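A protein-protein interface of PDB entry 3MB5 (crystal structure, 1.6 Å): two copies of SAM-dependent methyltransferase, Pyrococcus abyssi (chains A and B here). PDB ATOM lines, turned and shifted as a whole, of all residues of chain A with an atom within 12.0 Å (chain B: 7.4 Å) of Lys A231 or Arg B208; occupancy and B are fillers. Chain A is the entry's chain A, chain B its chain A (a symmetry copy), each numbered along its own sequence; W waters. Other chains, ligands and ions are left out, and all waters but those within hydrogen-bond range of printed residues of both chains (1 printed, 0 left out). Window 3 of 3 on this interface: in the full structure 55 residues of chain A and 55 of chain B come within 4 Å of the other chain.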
ATOM      1  N   GLN A 227     -25.729 -19.571 -19.108  1.00  0.00           N
ATOM      2  CA  GLN A 227     -24.859 -18.595 -18.451  1.00  0.00           C
ATOM      3  C   GLN A 227     -25.174 -17.199 -18.965  1.00  0.00           C
ATOM      4  O   GLN A 227     -25.356 -16.981 -20.174  1.00  0.00           O
ATOM      5  CB  GLN A 227     -23.383 -18.930 -18.722  1.00  0.00           C
ATOM      6  CG  GLN A 227     -22.913 -20.293 -18.170  1.00  0.00           C
ATOM      7  CD  GLN A 227     -22.912 -20.374 -16.623  1.00  0.00           C
ATOM      8  OE1 GLN A 227     -22.567 -19.422 -15.955  1.00  0.00           O
ATOM      9  NE2 GLN A 227     -23.244 -21.553 -16.073  1.00  0.00           N
ATOM     10  N   GLU A 228     -25.224 -16.240 -18.051  1.00  0.00           N
ATOM     11  CA  GLU A 228     -25.356 -14.837 -18.434  1.00  0.00           C
ATOM     12  C   GLU A 228     -23.976 -14.219 -18.424  1.00  0.00           C
ATOM     13  O   GLU A 228     -23.311 -14.227 -17.405  1.00  0.00           O
ATOM     14  CB  GLU A 228     -26.285 -14.120 -17.462  1.00  0.00           C
ATOM     15  CG  GLU A 228     -26.583 -12.669 -17.876  1.00  0.00           C
ATOM     16  CD  GLU A 228     -27.621 -12.018 -16.982  1.00  0.00           C
ATOM     17  OE1 GLU A 228     -27.277 -11.670 -15.831  1.00  0.00           O
ATOM     18  OE2 GLU A 228     -28.780 -11.860 -17.446  1.00  0.00           O
ATOM     19  N   VAL A 229     -23.518 -13.724 -19.572  1.00  0.00           N
ATOM     20  CA  VAL A 229     -22.157 -13.222 -19.684  1.00  0.00           C
ATOM     21  C   VAL A 229     -22.222 -11.765 -20.098  1.00  0.00           C
ATOM     22  O   VAL A 229     -22.309 -11.451 -21.284  1.00  0.00           O
ATOM     23  CB  VAL A 229     -21.316 -14.028 -20.726  1.00  0.00           C
ATOM     24  CG1 VAL A 229     -19.840 -13.664 -20.620  1.00  0.00           C
ATOM     25  CG2 VAL A 229     -21.517 -15.558 -20.538  1.00  0.00           C
ATOM     26  N   LYS A 230     -22.219 -10.882 -19.116  1.00  0.00           N
ATOM     27  CA  LYS A 230     -22.164  -9.441 -19.377  1.00  0.00           C
ATOM     28  C   LYS A 230     -20.740  -8.978 -19.149  1.00  0.00           C
ATOM     29  O   LYS A 230     -19.973  -9.636 -18.437  1.00  0.00           O
ATOM     30  CB  LYS A 230     -23.150  -8.690 -18.470  1.00  0.00           C
ATOM     31  CG  LYS A 230     -24.618  -9.033 -18.775  1.00  0.00           C
ATOM     32  CD  LYS A 230     -25.578  -8.195 -17.949  1.00  0.00           C
ATOM     33  CE  LYS A 230     -27.030  -8.573 -18.234  1.00  0.00           C
ATOM     34  NZ  LYS A 230     -27.525  -7.976 -19.516  1.00  0.00           N
ATOM     35  N   LYS A 231     -20.373  -7.841 -19.741  1.00  0.00           N
ATOM     36  CA  LYS A 231     -19.010  -7.330 -19.624  1.00  0.00           C
ATOM     37  C   LYS A 231     -18.485  -7.350 -18.188  1.00  0.00           C
ATOM     38  O   LYS A 231     -17.337  -7.708 -17.962  1.00  0.00           O
ATOM     39  CB  LYS A 231     -18.906  -5.912 -20.207  1.00  0.00           C
ATOM     40  CG  LYS A 231     -17.499  -5.342 -20.165  1.00  0.00           C
ATOM     41  CD  LYS A 231     -17.427  -3.933 -20.751  1.00  0.00           C
ATOM     42  CE  LYS A 231     -16.004  -3.403 -20.648  1.00  0.00           C
ATOM     43  NZ  LYS A 231     -15.837  -2.127 -21.404  1.00  0.00           N
ATOM     44  N   GLU A 232     -19.318  -6.996 -17.217  1.00  0.00           N
ATOM     45  CA  GLU A 232     -18.805  -6.893 -15.855  1.00  0.00           C
ATOM     46  C   GLU A 232     -19.298  -7.992 -14.927  1.00  0.00           C
ATOM     47  O   GLU A 232     -18.960  -7.986 -13.747  1.00  0.00           O
ATOM     48  CB  GLU A 232     -19.090  -5.514 -15.250  1.00  0.00           C
ATOM     49  CG  GLU A 232     -18.487  -4.313 -16.041  1.00  0.00           C
ATOM     50  CD  GLU A 232     -16.949  -4.229 -16.017  1.00  0.00           C
ATOM     51  OE1 GLU A 232     -16.408  -3.236 -16.562  1.00  0.00           O
ATOM     52  OE2 GLU A 232     -16.269  -5.130 -15.467  1.00  0.00           O
ATOM     53  N   CYS A 233     -20.075  -8.940 -15.457  1.00  0.00           N
ATOM     54  CA  CYS A 233     -20.669  -9.982 -14.616  1.00  0.00           C
ATOM     55  C   CYS A 233     -21.014 -11.228 -15.423  1.00  0.00           C
ATOM     56  O   CYS A 233     -21.941 -11.208 -16.225  1.00  0.00           O
ATOM     57  CB  CYS A 233     -21.943  -9.477 -13.950  1.00  0.00           C
ATOM     58  SG  CYS A 233     -22.703 -10.724 -12.822  1.00  0.00           S
ATOM     59  N   MET A 234     -20.284 -12.305 -15.171  1.00  0.00           N
ATOM     60  CA  MET A 234     -20.670 -13.620 -15.646  1.00  0.00           C
ATOM     61  C   MET A 234     -21.221 -14.429 -14.483  1.00  0.00           C
ATOM     62  O   MET A 234     -20.574 -14.512 -13.430  1.00  0.00           O
ATOM     63  CB  MET A 234     -19.488 -14.360 -16.258  1.00  0.00           C
ATOM     64  CG  MET A 234     -19.849 -15.803 -16.623  1.00  0.00           C
ATOM     65  SD  MET A 234     -18.508 -16.574 -17.516  1.00  0.00           S
ATOM     66  CE  MET A 234     -19.140 -18.257 -17.627  1.00  0.00           C
ATOM     67  N   ARG A 235     -22.414 -14.988 -14.668  1.00  0.00           N
ATOM     68  CA  ARG A 235     -23.014 -15.875 -13.664  1.00  0.00           C
ATOM     69  C   ARG A 235     -24.034 -16.759 -14.347  1.00  0.00           C
ATOM     70  O   ARG A 235     -24.543 -16.411 -15.409  1.00  0.00           O
ATOM     71  CB  ARG A 235     -23.698 -15.061 -12.564  1.00  0.00           C
ATOM     72  CG  ARG A 235     -24.723 -14.075 -13.125  1.00  0.00           C
ATOM     73  CD  ARG A 235     -25.406 -13.274 -12.049  1.00  0.00           C
ATOM     74  NE  ARG A 235     -26.277 -12.288 -12.678  1.00  0.00           N
ATOM     75  CZ  ARG A 235     -27.085 -11.461 -12.020  1.00  0.00           C
ATOM     76  NH1 ARG A 235     -27.154 -11.500 -10.692  1.00  0.00           N
ATOM     77  NH2 ARG A 235     -27.829 -10.591 -12.699  1.00  0.00           N
ATOM     78  N   VAL B 177     -12.809 -16.004 -34.303  1.00  0.00           N
ATOM     79  CA  VAL B 177     -14.124 -15.391 -34.576  1.00  0.00           C
ATOM     80  C   VAL B 177     -14.161 -14.689 -35.933  1.00  0.00           C
ATOM     81  O   VAL B 177     -15.058 -14.927 -36.713  1.00  0.00           O
ATOM     82  CB  VAL B 177     -14.567 -14.434 -33.441  1.00  0.00           C
ATOM     83  CG1 VAL B 177     -15.814 -13.655 -33.834  1.00  0.00           C
ATOM     84  CG2 VAL B 177     -14.819 -15.256 -32.157  1.00  0.00           C
ATOM     85  N   VAL B 200     -14.714 -18.010 -21.414  1.00  0.00           N
ATOM     86  CA  VAL B 200     -16.036 -17.581 -21.849  1.00  0.00           C
ATOM     87  C   VAL B 200     -16.085 -16.040 -21.898  1.00  0.00           C
ATOM     88  O   VAL B 200     -16.624 -15.464 -22.843  1.00  0.00           O
ATOM     89  CB  VAL B 200     -17.135 -18.140 -20.916  1.00  0.00           C
ATOM     90  CG1 VAL B 200     -18.508 -17.593 -21.274  1.00  0.00           C
ATOM     91  CG2 VAL B 200     -17.146 -19.664 -21.000  1.00  0.00           C
ATOM     92  N   MET B 201     -15.529 -15.405 -20.868  1.00  0.00           N
ATOM     93  CA  MET B 201     -15.487 -13.947 -20.798  1.00  0.00           C
ATOM     94  C   MET B 201     -14.739 -13.379 -21.997  1.00  0.00           C
ATOM     95  O   MET B 201     -15.251 -12.455 -22.635  1.00  0.00           O
ATOM     96  CB  MET B 201     -14.839 -13.492 -19.484  1.00  0.00           C
ATOM     97  CG  MET B 201     -15.632 -13.889 -18.239  1.00  0.00           C
ATOM     98  SD  MET B 201     -14.649 -13.471 -16.780  1.00  0.00           S
ATOM     99  CE  MET B 201     -15.831 -13.875 -15.481  1.00  0.00           C
ATOM    100  N   ARG B 202     -13.557 -13.917 -22.289  1.00  0.00           N
ATOM    101  CA  ARG B 202     -12.738 -13.414 -23.421  1.00  0.00           C
ATOM    102  C   ARG B 202     -13.446 -13.632 -24.746  1.00  0.00           C
ATOM    103  O   ARG B 202     -13.450 -12.761 -25.626  1.00  0.00           O
ATOM    104  CB  ARG B 202     -11.360 -14.058 -23.425  1.00  0.00           C
ATOM    105  CG  ARG B 202     -10.458 -13.529 -22.305  1.00  0.00           C
ATOM    106  CD  ARG B 202      -9.041 -14.033 -22.424  1.00  0.00           C
ATOM    107  NE  ARG B 202      -8.869 -15.459 -22.136  1.00  0.00           N
ATOM    108  CZ  ARG B 202      -8.640 -15.992 -20.935  1.00  0.00           C
ATOM    109  NH1 ARG B 202      -8.558 -15.233 -19.843  1.00  0.00           N
ATOM    110  NH2 ARG B 202      -8.472 -17.301 -20.829  1.00  0.00           N
ATOM    111  N   LEU B 203     -14.103 -14.779 -24.882  1.00  0.00           N
ATOM    112  CA  LEU B 203     -14.836 -15.065 -26.111  1.00  0.00           C
ATOM    113  C   LEU B 203     -16.007 -14.106 -26.334  1.00  0.00           C
ATOM    114  O   LEU B 203     -16.229 -13.623 -27.451  1.00  0.00           O
ATOM    115  CB  LEU B 203     -15.324 -16.525 -26.106  1.00  0.00           C
ATOM    116  CG  LEU B 203     -16.111 -16.974 -27.331  1.00  0.00           C
ATOM    117  CD1 LEU B 203     -15.343 -16.711 -28.632  1.00  0.00           C
ATOM    118  CD2 LEU B 203     -16.433 -18.468 -27.207  1.00  0.00           C
ATOM    119  N   HIS B 204     -16.763 -13.823 -25.275  1.00  0.00           N
ATOM    120  CA  HIS B 204     -17.895 -12.913 -25.379  1.00  0.00           C
ATOM    121  C   HIS B 204     -17.443 -11.480 -25.663  1.00  0.00           C
ATOM    122  O   HIS B 204     -18.159 -10.783 -26.344  1.00  0.00           O
ATOM    123  CB  HIS B 204     -18.767 -12.980 -24.128  1.00  0.00           C
ATOM    124  CG  HIS B 204     -19.785 -14.074 -24.185  1.00  0.00           C
ATOM    125  ND1 HIS B 204     -21.092 -13.842 -24.545  1.00  0.00           N
ATOM    126  CD2 HIS B 204     -19.690 -15.399 -23.921  1.00  0.00           C
ATOM    127  CE1 HIS B 204     -21.762 -14.984 -24.504  1.00  0.00           C
ATOM    128  NE2 HIS B 204     -20.929 -15.941 -24.147  1.00  0.00           N
ATOM    129  N   GLU B 205     -16.265 -11.089 -25.170  1.00  0.00           N
ATOM    130  CA  GLU B 205     -15.685  -9.767 -25.497  1.00  0.00           C
ATOM    131  C   GLU B 205     -15.515  -9.676 -27.015  1.00  0.00           C
ATOM    132  O   GLU B 205     -15.905  -8.676 -27.645  1.00  0.00           O
ATOM    133  CB  GLU B 205     -14.343  -9.545 -24.764  1.00  0.00           C
ATOM    134  CG  GLU B 205     -13.731  -8.155 -24.989  1.00  0.00           C
ATOM    135  CD  GLU B 205     -12.355  -7.991 -24.341  1.00  0.00           C
ATOM    136  OE1 GLU B 205     -12.059  -8.694 -23.348  1.00  0.00           O
ATOM    137  OE2 GLU B 205     -11.567  -7.145 -24.822  1.00  0.00           O
ATOM    138  N   LYS B 206     -14.991 -10.744 -27.602  1.00  0.00           N
ATOM    139  CA  LYS B 206     -14.745 -10.769 -29.051  1.00  0.00           C
ATOM    140  C   LYS B 206     -16.063 -10.863 -29.836  1.00  0.00           C
ATOM    141  O   LYS B 206     -16.262 -10.203 -30.858  1.00  0.00           O
ATOM    142  CB  LYS B 206     -13.790 -11.904 -29.380  1.00  0.00           C
ATOM    143  CG  LYS B 206     -13.486 -12.068 -30.866  1.00  0.00           C
ATOM    144  CD  LYS B 206     -12.789 -10.819 -31.445  1.00  0.00           C
ATOM    145  CE  LYS B 206     -11.361 -10.670 -30.927  1.00  0.00           C
ATOM    146  NZ  LYS B 206     -10.728  -9.506 -31.660  1.00  0.00           N
ATOM    147  N   LEU B 207     -17.005 -11.655 -29.344  1.00  0.00           N
ATOM    148  CA  LEU B 207     -18.291 -11.715 -30.006  1.00  0.00           C
ATOM    149  C   LEU B 207     -19.055 -10.368 -29.975  1.00  0.00           C
ATOM    150  O   LEU B 207     -19.756 -10.062 -30.931  1.00  0.00           O
ATOM    151  CB  LEU B 207     -19.142 -12.857 -29.410  1.00  0.00           C
ATOM    152  CG  LEU B 207     -18.669 -14.263 -29.763  1.00  0.00           C
ATOM    153  CD1 LEU B 207     -19.371 -15.287 -28.834  1.00  0.00           C
ATOM    154  CD2 LEU B 207     -18.915 -14.625 -31.221  1.00  0.00           C
ATOM    155  N   ARG B 208     -18.914  -9.598 -28.886  1.00  0.00           N
ATOM    156  CA  ARG B 208     -19.518  -8.235 -28.781  1.00  0.00           C
ATOM    157  C   ARG B 208     -18.891  -7.327 -29.842  1.00  0.00           C
ATOM    158  O   ARG B 208     -19.598  -6.558 -30.498  1.00  0.00           O
ATOM    159  CB  ARG B 208     -19.314  -7.613 -27.393  1.00  0.00           C
ATOM    160  CG  ARG B 208     -20.213  -8.197 -26.293  1.00  0.00           C
ATOM    161  CD  ARG B 208     -20.168  -7.442 -24.931  1.00  0.00           C
ATOM    162  NE  ARG B 208     -18.843  -7.257 -24.328  1.00  0.00           N
ATOM    163  CZ  ARG B 208     -18.284  -8.085 -23.435  1.00  0.00           C
ATOM    164  NH1 ARG B 208     -18.917  -9.182 -23.031  1.00  0.00           N
ATOM    165  NH2 ARG B 208     -17.079  -7.810 -22.938  1.00  0.00           N
ATOM    166  N   GLU B 209     -17.573  -7.418 -29.994  1.00  0.00           N
ATOM    167  CA  GLU B 209     -16.881  -6.673 -31.056  1.00  0.00           C
ATOM    168  C   GLU B 209     -17.456  -7.028 -32.418  1.00  0.00           C
ATOM    169  O   GLU B 209     -17.592  -6.150 -33.295  1.00  0.00           O
ATOM    170  CB  GLU B 209     -15.373  -6.936 -31.019  1.00  0.00           C
ATOM    171  CG  GLU B 209     -14.579  -6.236 -32.137  1.00  0.00           C
ATOM    172  CD  GLU B 209     -13.095  -6.576 -32.128  1.00  0.00           C
ATOM    173  OE1 GLU B 209     -12.353  -5.998 -32.953  1.00  0.00           O
ATOM    174  OE2 GLU B 209     -12.660  -7.420 -31.322  1.00  0.00           O
ATOM    175  N   PHE B 210     -17.805  -8.305 -32.595  1.00  0.00           N
ATOM    176  CA  PHE B 210     -18.349  -8.807 -33.867  1.00  0.00           C
ATOM    177  C   PHE B 210     -19.874  -8.955 -33.842  1.00  0.00           C
ATOM    178  O   PHE B 210     -20.435  -9.786 -34.553  1.00  0.00           O
ATOM    179  CB  PHE B 210     -17.650 -10.127 -34.259  1.00  0.00           C
ATOM    180  CG  PHE B 210     -16.319  -9.914 -34.928  1.00  0.00           C
ATOM    181  CD1 PHE B 210     -15.181  -9.613 -34.187  1.00  0.00           C
ATOM    182  CD2 PHE B 210     -16.216  -9.996 -36.322  1.00  0.00           C
ATOM    183  CE1 PHE B 210     -13.950  -9.388 -34.815  1.00  0.00           C
ATOM    184  CE2 PHE B 210     -14.990  -9.765 -36.969  1.00  0.00           C
ATOM    185  CZ  PHE B 210     -13.862  -9.466 -36.220  1.00  0.00           C
ATOM    186  N   LYS B 211     -20.542  -8.128 -33.036  1.00  0.00           N
ATOM    187  CA  LYS B 211     -21.996  -8.250 -32.832  1.00  0.00           C
ATOM    188  C   LYS B 211     -22.845  -8.195 -34.113  1.00  0.00           C
ATOM    189  O   LYS B 211     -23.900  -8.833 -34.178  1.00  0.00           O
ATOM    190  CB  LYS B 211     -22.494  -7.230 -31.804  1.00  0.00           C
ATOM    191  CG  LYS B 211     -22.566  -5.793 -32.323  1.00  0.00           C
ATOM    192  CD  LYS B 211     -22.671  -4.786 -31.185  1.00  0.00           C
ATOM    193  CE  LYS B 211     -23.772  -5.131 -30.188  1.00  0.00           C
ATOM    194  NZ  LYS B 211     -23.880  -4.096 -29.111  1.00  0.00           N
ATOM    195  N   ASP B 212     -22.373  -7.463 -35.120  1.00  0.00           N
ATOM    196  CA  ASP B 212     -23.094  -7.290 -36.398  1.00  0.00           C
ATOM    197  C   ASP B 212     -22.806  -8.416 -37.390  1.00  0.00           C
ATOM    198  O   ASP B 212     -23.150  -8.334 -38.592  1.00  0.00           O
ATOM    199  CB  ASP B 212     -22.735  -5.947 -37.049  1.00  0.00           C
ATOM    200  CG  ASP B 212     -23.100  -4.744 -36.184  1.00  0.00           C
ATOM    201  OD1 ASP B 212     -24.041  -4.827 -35.352  1.00  0.00           O
ATOM    202  OD2 ASP B 212     -22.432  -3.702 -36.359  1.00  0.00           O
ATOM    203  N   PHE B 214     -23.093 -11.761 -36.040  1.00  0.00           N
ATOM    204  CA  PHE B 214     -23.782 -12.895 -35.412  1.00  0.00           C
ATOM    205  C   PHE B 214     -25.095 -12.511 -34.740  1.00  0.00           C
ATOM    206  O   PHE B 214     -25.313 -11.345 -34.365  1.00  0.00           O
ATOM    207  CB  PHE B 214     -22.873 -13.551 -34.361  1.00  0.00           C
ATOM    208  CG  PHE B 214     -21.622 -14.127 -34.926  1.00  0.00           C
ATOM    209  CD1 PHE B 214     -20.452 -13.370 -34.951  1.00  0.00           C
ATOM    210  CD2 PHE B 214     -21.605 -15.426 -35.475  1.00  0.00           C
ATOM    211  CE1 PHE B 214     -19.281 -13.868 -35.494  1.00  0.00           C
ATOM    212  CE2 PHE B 214     -20.422 -15.957 -36.004  1.00  0.00           C
ATOM    213  CZ  PHE B 214     -19.248 -15.164 -36.037  1.00  0.00           C
ATOM    214  N   PRO B 217     -25.240 -14.469 -28.945  1.00  0.00           N
ATOM    215  CA  PRO B 217     -24.605 -15.715 -28.519  1.00  0.00           C
ATOM    216  C   PRO B 217     -25.239 -16.299 -27.278  1.00  0.00           C
ATOM    217  O   PRO B 217     -25.876 -15.584 -26.509  1.00  0.00           O
ATOM    218  CB  PRO B 217     -23.164 -15.309 -28.216  1.00  0.00           C
ATOM    219  CG  PRO B 217     -23.215 -13.858 -27.935  1.00  0.00           C
ATOM    220  CD  PRO B 217     -24.376 -13.296 -28.691  1.00  0.00           C
HETATM  221  O   HOH W   1     -21.541 -10.066 -23.441  1.00  0.00           O
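Water W1 lies within hydrogen-bond range of the backbone carbonyl oxygen (O) of Val A229 (2.7 Å) and the guanidinium group (NH1) of Arg B208 (2.8 Å).
Along chain B the printed residues that touch a printed residue of chain A span positions 200 to 208.
Among the printed residues, no Asp or Glu carboxylate lies within 4 Å of a Lys or Arg side-chain nitrogen of the other chain.
No position is printed for both chains.
Among the printed residues, merely in contact across the chains: Val A229 with Val B200 (3.7 Å), Val A229 with His B204 (3.6 Å), Lys A231 with Arg B208 (3.7 Å), Met A234 with Val B200 (3.8 Å) and Met A234 with Met B201 (3.8 Å).
Lys A231 touches one residue of chain B.
Of chain A, only Lys A231 comes within 4 Å of Arg B208.
Of chain A, only Met A234 comes within 4 Å of Met B201.
His B204 touches one residue of chain A.
No residue of chain A comes within 4 Å of Leu B207.
No residue of chain A comes within 4 Å of Lys B211.
Of the printed residues of chain A, Val B200 touches Val A229 (3.7 Å) and Met A234 (3.8 Å).
Of the printed residues of chain B, Met A234 touches Val B200 (3.8 Å) and Met B201 (3.8 Å).
Printed residues of chain B within 4 Å of Val A229: Val B200 (3.7 Å) and His B204 (3.6 Å).
Arg A235 touches none of the printed residues of chain B.
The nearest residue of chain B that does not touch Lys A231 is Met B201 (6.4 Å).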
